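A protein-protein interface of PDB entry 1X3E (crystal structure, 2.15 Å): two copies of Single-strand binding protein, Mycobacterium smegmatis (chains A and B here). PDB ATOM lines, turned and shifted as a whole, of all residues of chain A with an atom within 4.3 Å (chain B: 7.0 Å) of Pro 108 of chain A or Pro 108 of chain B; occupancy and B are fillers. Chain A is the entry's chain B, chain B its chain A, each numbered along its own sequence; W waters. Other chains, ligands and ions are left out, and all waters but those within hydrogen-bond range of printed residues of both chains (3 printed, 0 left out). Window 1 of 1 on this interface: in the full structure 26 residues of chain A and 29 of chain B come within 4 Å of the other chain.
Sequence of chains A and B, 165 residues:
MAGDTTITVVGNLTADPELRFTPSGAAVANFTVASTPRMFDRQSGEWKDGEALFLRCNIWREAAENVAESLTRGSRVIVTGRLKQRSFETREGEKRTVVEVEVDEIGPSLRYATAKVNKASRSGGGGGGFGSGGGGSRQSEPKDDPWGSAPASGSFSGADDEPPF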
ATOM      1  N   LEU A  71     -16.771   7.074   7.409  1.00  0.00           N
ATOM      2  CA  LEU A  71     -17.220   5.889   6.669  1.00  0.00           C
ATOM      3  C   LEU A  71     -18.586   6.126   6.030  1.00  0.00           C
ATOM      4  O   LEU A  71     -19.370   6.944   6.493  1.00  0.00           O
ATOM      5  CB  LEU A  71     -17.275   4.671   7.595  1.00  0.00           C
ATOM      6  CG  LEU A  71     -16.007   4.332   8.403  1.00  0.00           C
ATOM      7  CD1 LEU A  71     -16.238   3.049   9.207  1.00  0.00           C
ATOM      8  CD2 LEU A  71     -14.799   4.160   7.458  1.00  0.00           C
ATOM      9  N   ARG A  76     -15.143  -0.539   2.910  1.00  0.00           N
ATOM     10  CA  ARG A  76     -14.556  -1.785   3.384  1.00  0.00           C
ATOM     11  C   ARG A  76     -13.925  -1.510   4.714  1.00  0.00           C
ATOM     12  O   ARG A  76     -13.176  -0.572   4.854  1.00  0.00           O
ATOM     13  CB  ARG A  76     -13.495  -2.283   2.423  1.00  0.00           C
ATOM     14  CG  ARG A  76     -12.856  -3.594   2.860  1.00  0.00           C
ATOM     15  CD  ARG A  76     -11.807  -4.121   1.916  1.00  0.00           C
ATOM     16  NE  ARG A  76     -12.441  -5.136   1.129  1.00  0.00           N
ATOM     17  CZ  ARG A  76     -12.449  -6.424   1.401  1.00  0.00           C
ATOM     18  NH1 ARG A  76     -13.118  -7.222   0.617  1.00  0.00           N
ATOM     19  NH2 ARG A  76     -11.775  -6.924   2.392  1.00  0.00           N
ATOM     20  N   ILE A 106     -12.376  -0.054  14.977  1.00  0.00           N
ATOM     21  CA  ILE A 106     -12.773  -0.181  13.575  1.00  0.00           C
ATOM     22  C   ILE A 106     -11.967   0.796  12.742  1.00  0.00           C
ATOM     23  O   ILE A 106     -11.649   1.890  13.194  1.00  0.00           O
ATOM     24  CB  ILE A 106     -14.270   0.126  13.393  1.00  0.00           C
ATOM     25  CG1 ILE A 106     -14.611   0.107  11.899  1.00  0.00           C
ATOM     26  CG2 ILE A 106     -14.636   1.501  14.038  1.00  0.00           C
ATOM     27  CD1 ILE A 106     -16.034   0.001  11.632  1.00  0.00           C
ATOM     28  N   GLY A 107     -11.681   0.412  11.506  1.00  0.00           N
ATOM     29  CA  GLY A 107     -10.966   1.258  10.555  1.00  0.00           C
ATOM     30  C   GLY A 107     -11.209   0.859   9.103  1.00  0.00           C
ATOM     31  O   GLY A 107     -11.568  -0.280   8.823  1.00  0.00           O
ATOM     32  N   PRO A 108     -11.029   1.790   8.167  1.00  0.00           N
ATOM     33  CA  PRO A 108     -11.190   1.449   6.743  1.00  0.00           C
ATOM     34  C   PRO A 108     -10.021   0.588   6.261  1.00  0.00           C
ATOM     35  O   PRO A 108      -8.857   0.912   6.533  1.00  0.00           O
ATOM     36  CB  PRO A 108     -11.214   2.817   6.051  1.00  0.00           C
ATOM     37  CG  PRO A 108     -10.401   3.700   6.937  1.00  0.00           C
ATOM     38  CD  PRO A 108     -10.683   3.219   8.358  1.00  0.00           C
ATOM     39  N   SER A 109     -10.319  -0.523   5.603  1.00  0.00           N
ATOM     40  CA  SER A 109      -9.257  -1.350   5.046  1.00  0.00           C
ATOM     41  C   SER A 109      -8.520  -0.604   3.939  1.00  0.00           C
ATOM     42  O   SER A 109      -9.135   0.069   3.137  1.00  0.00           O
ATOM     43  CB  SER A 109      -9.807  -2.651   4.463  1.00  0.00           C
ATOM     44  OG  SER A 109      -8.774  -3.318   3.798  1.00  0.00           O
ATOM     45  N   LEU A 110      -7.209  -0.791   3.891  1.00  0.00           N
ATOM     46  CA  LEU A 110      -6.368  -0.250   2.851  1.00  0.00           C
ATOM     47  C   LEU A 110      -6.137  -1.213   1.667  1.00  0.00           C
ATOM     48  O   LEU A 110      -5.293  -0.984   0.802  1.00  0.00           O
ATOM     49  CB  LEU A 110      -5.042   0.177   3.473  1.00  0.00           C
ATOM     50  CG  LEU A 110      -5.179   1.270   4.530  1.00  0.00           C
ATOM     51  CD1 LEU A 110      -3.777   1.777   4.886  1.00  0.00           C
ATOM     52  CD2 LEU A 110      -6.078   2.430   4.102  1.00  0.00           C
ATOM     53  N   VAL A 117      -5.267  10.137   7.235  1.00  0.00           N
ATOM     54  CA  VAL A 117      -5.585   9.943   8.626  1.00  0.00           C
ATOM     55  C   VAL A 117      -5.347  11.251   9.330  1.00  0.00           C
ATOM     56  O   VAL A 117      -4.339  11.899   9.103  1.00  0.00           O
ATOM     57  CB  VAL A 117      -4.704   8.823   9.259  1.00  0.00           C
ATOM     58  CG1 VAL A 117      -4.905   8.738  10.772  1.00  0.00           C
ATOM     59  CG2 VAL A 117      -5.021   7.481   8.637  1.00  0.00           C
ATOM     60  N   SER B  70      -0.560   5.833   3.098  1.00  0.00           N
ATOM     61  CA  SER B  70      -1.577   6.235   4.071  1.00  0.00           C
ATOM     62  C   SER B  70      -1.087   6.261   5.508  1.00  0.00           C
ATOM     63  O   SER B  70      -1.660   6.959   6.318  1.00  0.00           O
ATOM     64  CB  SER B  70      -2.800   5.301   4.014  1.00  0.00           C
ATOM     65  OG  SER B  70      -3.301   5.165   2.688  1.00  0.00           O
ATOM     66  N   LEU B  71      -0.050   5.496   5.843  1.00  0.00           N
ATOM     67  CA  LEU B  71       0.342   5.315   7.242  1.00  0.00           C
ATOM     68  C   LEU B  71       1.760   5.808   7.478  1.00  0.00           C
ATOM     69  O   LEU B  71       2.600   5.792   6.577  1.00  0.00           O
ATOM     70  CB  LEU B  71       0.261   3.841   7.634  1.00  0.00           C
ATOM     71  CG  LEU B  71      -1.113   3.186   7.485  1.00  0.00           C
ATOM     72  CD1 LEU B  71      -1.021   1.734   7.860  1.00  0.00           C
ATOM     73  CD2 LEU B  71      -2.189   3.886   8.320  1.00  0.00           C
ATOM     74  N   SER B  75       1.005   5.911  13.555  1.00  0.00           N
ATOM     75  CA  SER B  75      -0.340   5.645  13.089  1.00  0.00           C
ATOM     76  C   SER B  75      -0.893   4.452  13.822  1.00  0.00           C
ATOM     77  O   SER B  75      -0.239   3.413  13.887  1.00  0.00           O
ATOM     78  CB  SER B  75      -0.369   5.304  11.594  1.00  0.00           C
ATOM     79  OG  SER B  75       0.109   6.362  10.814  1.00  0.00           O
ATOM     80  N   ARG B  76      -2.101   4.606  14.358  1.00  0.00           N
ATOM     81  CA  ARG B  76      -2.789   3.537  15.061  1.00  0.00           C
ATOM     82  C   ARG B  76      -3.527   2.694  14.056  1.00  0.00           C
ATOM     83  O   ARG B  76      -4.283   3.200  13.225  1.00  0.00           O
ATOM     84  CB  ARG B  76      -3.745   4.103  16.092  1.00  0.00           C
ATOM     85  CG  ARG B  76      -4.257   3.078  17.082  1.00  0.00           C
ATOM     86  CD  ARG B  76      -5.402   3.583  17.919  1.00  0.00           C
ATOM     87  NE  ARG B  76      -5.998   2.563  18.775  1.00  0.00           N
ATOM     88  CZ  ARG B  76      -5.481   2.189  19.949  1.00  0.00           C
ATOM     89  NH1 ARG B  76      -6.077   1.268  20.704  1.00  0.00           N
ATOM     90  NH2 ARG B  76      -4.347   2.723  20.375  1.00  0.00           N
ATOM     91  N   VAL B  77      -3.285   1.398  14.114  1.00  0.00           N
ATOM     92  CA  VAL B  77      -3.739   0.478  13.100  1.00  0.00           C
ATOM     93  C   VAL B  77      -4.367  -0.754  13.687  1.00  0.00           C
ATOM     94  O   VAL B  77      -4.081  -1.148  14.800  1.00  0.00           O
ATOM     95  CB  VAL B  77      -2.575   0.047  12.144  1.00  0.00           C
ATOM     96  CG1 VAL B  77      -1.963   1.236  11.446  1.00  0.00           C
ATOM     97  CG2 VAL B  77      -1.485  -0.712  12.862  1.00  0.00           C
ATOM     98  N   ILE B  78      -5.240  -1.358  12.902  1.00  0.00           N
ATOM     99  CA  ILE B  78      -5.846  -2.646  13.202  1.00  0.00           C
ATOM    100  C   ILE B  78      -5.318  -3.580  12.120  1.00  0.00           C
ATOM    101  O   ILE B  78      -5.472  -3.287  10.945  1.00  0.00           O
ATOM    102  CB  ILE B  78      -7.371  -2.556  13.108  1.00  0.00           C
ATOM    103  CG1 ILE B  78      -7.884  -1.411  13.981  1.00  0.00           C
ATOM    104  CG2 ILE B  78      -8.035  -3.878  13.541  1.00  0.00           C
ATOM    105  CD1 ILE B  78      -9.313  -1.027  13.698  1.00  0.00           C
ATOM    106  N   ILE B 106      -5.470  -4.569   6.831  1.00  0.00           N
ATOM    107  CA  ILE B 106      -4.970  -3.549   7.731  1.00  0.00           C
ATOM    108  C   ILE B 106      -5.757  -2.280   7.435  1.00  0.00           C
ATOM    109  O   ILE B 106      -6.063  -1.975   6.278  1.00  0.00           O
ATOM    110  CB  ILE B 106      -3.434  -3.287   7.556  1.00  0.00           C
ATOM    111  CG1 ILE B 106      -2.998  -2.094   8.406  1.00  0.00           C
ATOM    112  CG2 ILE B 106      -3.077  -2.985   6.096  1.00  0.00           C
ATOM    113  CD1 ILE B 106      -1.527  -2.010   8.631  1.00  0.00           C
ATOM    114  N   GLY B 107      -6.042  -1.531   8.493  1.00  0.00           N
ATOM    115  CA  GLY B 107      -6.646  -0.210   8.362  1.00  0.00           C
ATOM    116  C   GLY B 107      -6.275   0.648   9.539  1.00  0.00           C
ATOM    117  O   GLY B 107      -5.957   0.098  10.615  1.00  0.00           O
ATOM    118  N   PRO B 108      -6.293   1.970   9.380  1.00  0.00           N
ATOM    119  CA  PRO B 108      -6.051   2.841  10.528  1.00  0.00           C
ATOM    120  C   PRO B 108      -7.287   2.844  11.392  1.00  0.00           C
ATOM    121  O   PRO B 108      -8.404   2.884  10.884  1.00  0.00           O
ATOM    122  CB  PRO B 108      -5.777   4.215   9.893  1.00  0.00           C
ATOM    123  CG  PRO B 108      -6.529   4.173   8.610  1.00  0.00           C
ATOM    124  CD  PRO B 108      -6.546   2.755   8.158  1.00  0.00           C
ATOM    125  N   SER B 109      -7.081   2.748  12.690  1.00  0.00           N
ATOM    126  CA  SER B 109      -8.184   2.788  13.648  1.00  0.00           C
ATOM    127  C   SER B 109      -8.813   4.173  13.697  1.00  0.00           C
ATOM    128  O   SER B 109      -8.109   5.178  13.627  1.00  0.00           O
ATOM    129  CB  SER B 109      -7.689   2.446  15.040  1.00  0.00           C
ATOM    130  OG  SER B 109      -8.786   2.436  15.929  1.00  0.00           O
ATOM    131  N   LEU B 110     -10.129   4.190  13.853  1.00  0.00           N
ATOM    132  CA  LEU B 110     -10.924   5.402  13.998  1.00  0.00           C
ATOM    133  C   LEU B 110     -11.294   5.660  15.459  1.00  0.00           C
ATOM    134  O   LEU B 110     -12.186   6.476  15.792  1.00  0.00           O
ATOM    135  CB  LEU B 110     -12.190   5.272  13.150  1.00  0.00           C
ATOM    136  CG  LEU B 110     -11.918   5.099  11.646  1.00  0.00           C
ATOM    137  CD1 LEU B 110     -13.201   4.932  10.920  1.00  0.00           C
ATOM    138  CD2 LEU B 110     -11.188   6.300  11.070  1.00  0.00           C
ATOM    139  N   ARG B 111     -10.593   4.989  16.348  1.00  0.00           N
ATOM    140  CA  ARG B 111     -10.837   5.182  17.762  1.00  0.00           C
ATOM    141  C   ARG B 111     -10.478   6.606  18.204  1.00  0.00           C
ATOM    142  O   ARG B 111     -11.197   7.235  18.947  1.00  0.00           O
ATOM    143  CB  ARG B 111     -10.027   4.169  18.571  1.00  0.00           C
ATOM    144  CG  ARG B 111     -10.152   4.406  20.061  1.00  0.00           C
ATOM    145  CD  ARG B 111     -10.590   3.188  20.823  1.00  0.00           C
ATOM    146  NE  ARG B 111      -9.565   2.653  21.686  1.00  0.00           N
ATOM    147  CZ  ARG B 111      -9.760   1.662  22.563  1.00  0.00           C
ATOM    148  NH1 ARG B 111     -10.960   1.079  22.685  1.00  0.00           N
ATOM    149  NH2 ARG B 111      -8.746   1.237  23.316  1.00  0.00           N
ATOM    150  N   ALA B 113      -9.135   8.901  15.810  1.00  0.00           N
ATOM    151  CA  ALA B 113      -8.865   9.619  14.577  1.00  0.00           C
ATOM    152  C   ALA B 113      -9.981   9.471  13.573  1.00  0.00           C
ATOM    153  O   ALA B 113     -10.797   8.559  13.638  1.00  0.00           O
ATOM    154  CB  ALA B 113      -7.563   9.141  13.939  1.00  0.00           C
ATOM    155  N   THR B 114     -10.001  10.407  12.645  1.00  0.00           N
ATOM    156  CA  THR B 114     -10.877  10.327  11.503  1.00  0.00           C
ATOM    157  C   THR B 114     -10.021  10.042  10.299  1.00  0.00           C
ATOM    158  O   THR B 114      -8.791  10.208  10.344  1.00  0.00           O
ATOM    159  CB  THR B 114     -11.626  11.651  11.328  1.00  0.00           C
ATOM    160  OG1 THR B 114     -10.687  12.717  11.117  1.00  0.00           O
ATOM    161  CG2 THR B 114     -12.339  12.017  12.621  1.00  0.00           C
ATOM    162  N   ALA B 115     -10.669   9.647   9.204  1.00  0.00           N
ATOM    163  CA  ALA B 115      -9.965   9.449   7.953  1.00  0.00           C
ATOM    164  C   ALA B 115     -10.805   9.807   6.724  1.00  0.00           C
ATOM    165  O   ALA B 115     -12.021   9.593   6.662  1.00  0.00           O
ATOM    166  CB  ALA B 115      -9.453   8.044   7.870  1.00  0.00           C
ATOM    167  N   LYS B 116     -10.152  10.406   5.747  1.00  0.00           N
ATOM    168  CA  LYS B 116     -10.778  10.630   4.466  1.00  0.00           C
ATOM    169  C   LYS B 116     -10.369   9.407   3.664  1.00  0.00           C
ATOM    170  O   LYS B 116      -9.189   9.171   3.492  1.00  0.00           O
ATOM    171  CB  LYS B 116     -10.258  11.925   3.824  1.00  0.00           C
ATOM    172  N   VAL B 117     -11.338   8.629   3.204  1.00  0.00           N
ATOM    173  CA  VAL B 117     -11.069   7.397   2.496  1.00  0.00           C
ATOM    174  C   VAL B 117     -11.306   7.568   1.006  1.00  0.00           C
ATOM    175  O   VAL B 117     -12.262   8.214   0.586  1.00  0.00           O
ATOM    176  CB  VAL B 117     -11.935   6.238   3.034  1.00  0.00           C
ATOM    177  CG1 VAL B 117     -11.544   4.945   2.374  1.00  0.00           C
ATOM    178  CG2 VAL B 117     -11.770   6.094   4.537  1.00  0.00           C
HETATM  179  O   HOH W   1     -12.314   2.626  16.537  1.00  0.00           O
HETATM  180  O   HOH W   2      -5.743  -4.113   3.970  1.00  0.00           O
HETATM  181  O   HOH W   3      -2.443   9.648   6.435  1.00  0.00           O
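Of chain B, only Gly 107 (3.1 Å), Pro 108 (3.4 Å), Leu 110 (3.98 Å) and Val 117 (3.7 Å) come within 4 Å of Pro 108 of chain A.
Of chain A, only Gly 107 (3.1 Å), Pro 108 (3.4 Å) and Val 117 (3.6 Å) come within 4 Å of Pro 108 of chain B.
Of the printed residues of chain A, Leu 110 of chain B touches Leu 71 (3.8 Å), Ile 106 (2.8 Å) and Pro 108 (3.98 Å).
Printed residues of chain B within 4 Å of Gly 107 of chain A: Ile 78 (3.5 Å) and Pro 108 (3.1 Å).
Of the printed residues of chain A, Thr 114 of chain B touches Val 117 (3.6 Å).
Of the printed residues of chain A, Ile 106 of chain B touches Ser 109 and Leu 110.
Of the printed residues of chain B, Ser 109 of chain A touches Ile 106 (3.5 Å).
The nearest residue of chain B that does not touch Pro 108 of chain A is Ile 106 of chain B (4.03 Å).
The nearest printed residue of chain B that does not touch Ile 106 of chain A is Pro 108 of chain B (4.1 Å).
N of Leu 110 of chain A is in hydrogen-bond range of O of Ile 106 of chain B, 2.9 Å away.
The backbone carbonyl oxygen (O) of Ile 106 of chain A is in hydrogen-bond range of the backbone NH (N) of Leu 110 of chain B (2.8 Å).
Ile 106 of chain A touches Ser 109 of chain B, and with the chains exchanged Ser 109 of chain A touches Ile 106 of chain B.
Gly 107 of chain A touches Pro 108 of chain B, and with the chains exchanged Pro 108 of chain A touches Gly 107 of chain B.
Pro 108 of chain B touches its own counterpart, Pro 108 of chain A.
Pro 108 of chain A touches Leu 110 of chain B, but with the chains exchanged Leu 110 of chain A does not touch Pro 108 of chain B (4.1 Å).
Positions printed for both chains: 71, 76, 106, 107, 108, 109, 110 and 117.
Among the printed residues, pairs that only touch across the chains: Gly 107 of chain A with Pro 108 of chain B (3.1 Å), Pro 108 of chain A with Gly 107 of chain B (3.1 Å), Ile 106 of chain A with Ile 78 of chain B (3.4 Å), Pro 108 of chain A with Pro 108 of chain B (3.4 Å), Ser 109 of chain A with Ile 106 of chain B (3.5 Å), Gly 107 of chain A with Ile 78 of chain B (3.5 Å), Val 117 of chain A with Pro 108 of chain B (3.6 Å), Ile 106 of chain A with Ser 109 of chain B (3.6 Å), Val 117 of chain A with Thr 114 of chain B (3.6 Å), Pro 108 of chain A with Val 117 of chain B (3.7 Å), Leu 110 of chain A with Ser 70 of chain B (3.8 Å), Leu 71 of chain A with Leu 110 of chain B (3.8 Å), Leu 110 of chain A with Leu 71 of chain B (3.98 Å) and Pro 108 of chain A with Leu 110 of chain B (3.98 Å).
Printed residues of chain A that touch a printed residue of chain B: Leu 71, Ile 106, Gly 107, Pro 108, Ser 109, Leu 110 and Val 117.
Along chain A the printed residues that touch a printed residue of chain B span positions 71 to 117.
Among the printed residues, no Asp or Glu carboxylate lies within 4 Å of a Lys or Arg side-chain nitrogen of the other chain.
Water W3 bridges the backbone carbonyl oxygen (O) of Ser 70 of chain B (2.8 Å) and the backbone NH (N) of Val 117 of chain A (3.0 Å).
Water W2 bridges N of Ile 106 of chain B (2.9 Å) and OG of Ser 109 of chain A (3.1 Å).
Water W1 bridges N of Arg 111 of chain B and N of Ile 106 of chain A.
The backbone carbonyl oxygen of Gly 107 of chain B sits at hydrogen-bond distance from the backbone NH of Ile 78 of chain B (2.8 Å).
The backbone NH (N) of Ser 109 of chain B sits at hydrogen-bond distance from the backbone carbonyl oxygen (O) of Arg 76 of chain B.
The side-chain hydroxyl (OG) of Ser 109 of chain B sits at hydrogen-bond distance from the backbone NH (N) of Arg 111 of chain B (3.2 Å).
The backbone NH of Ser 109 of chain A sits at hydrogen-bond distance from the backbone carbonyl oxygen of Arg 76 of chain A (3.0 Å).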
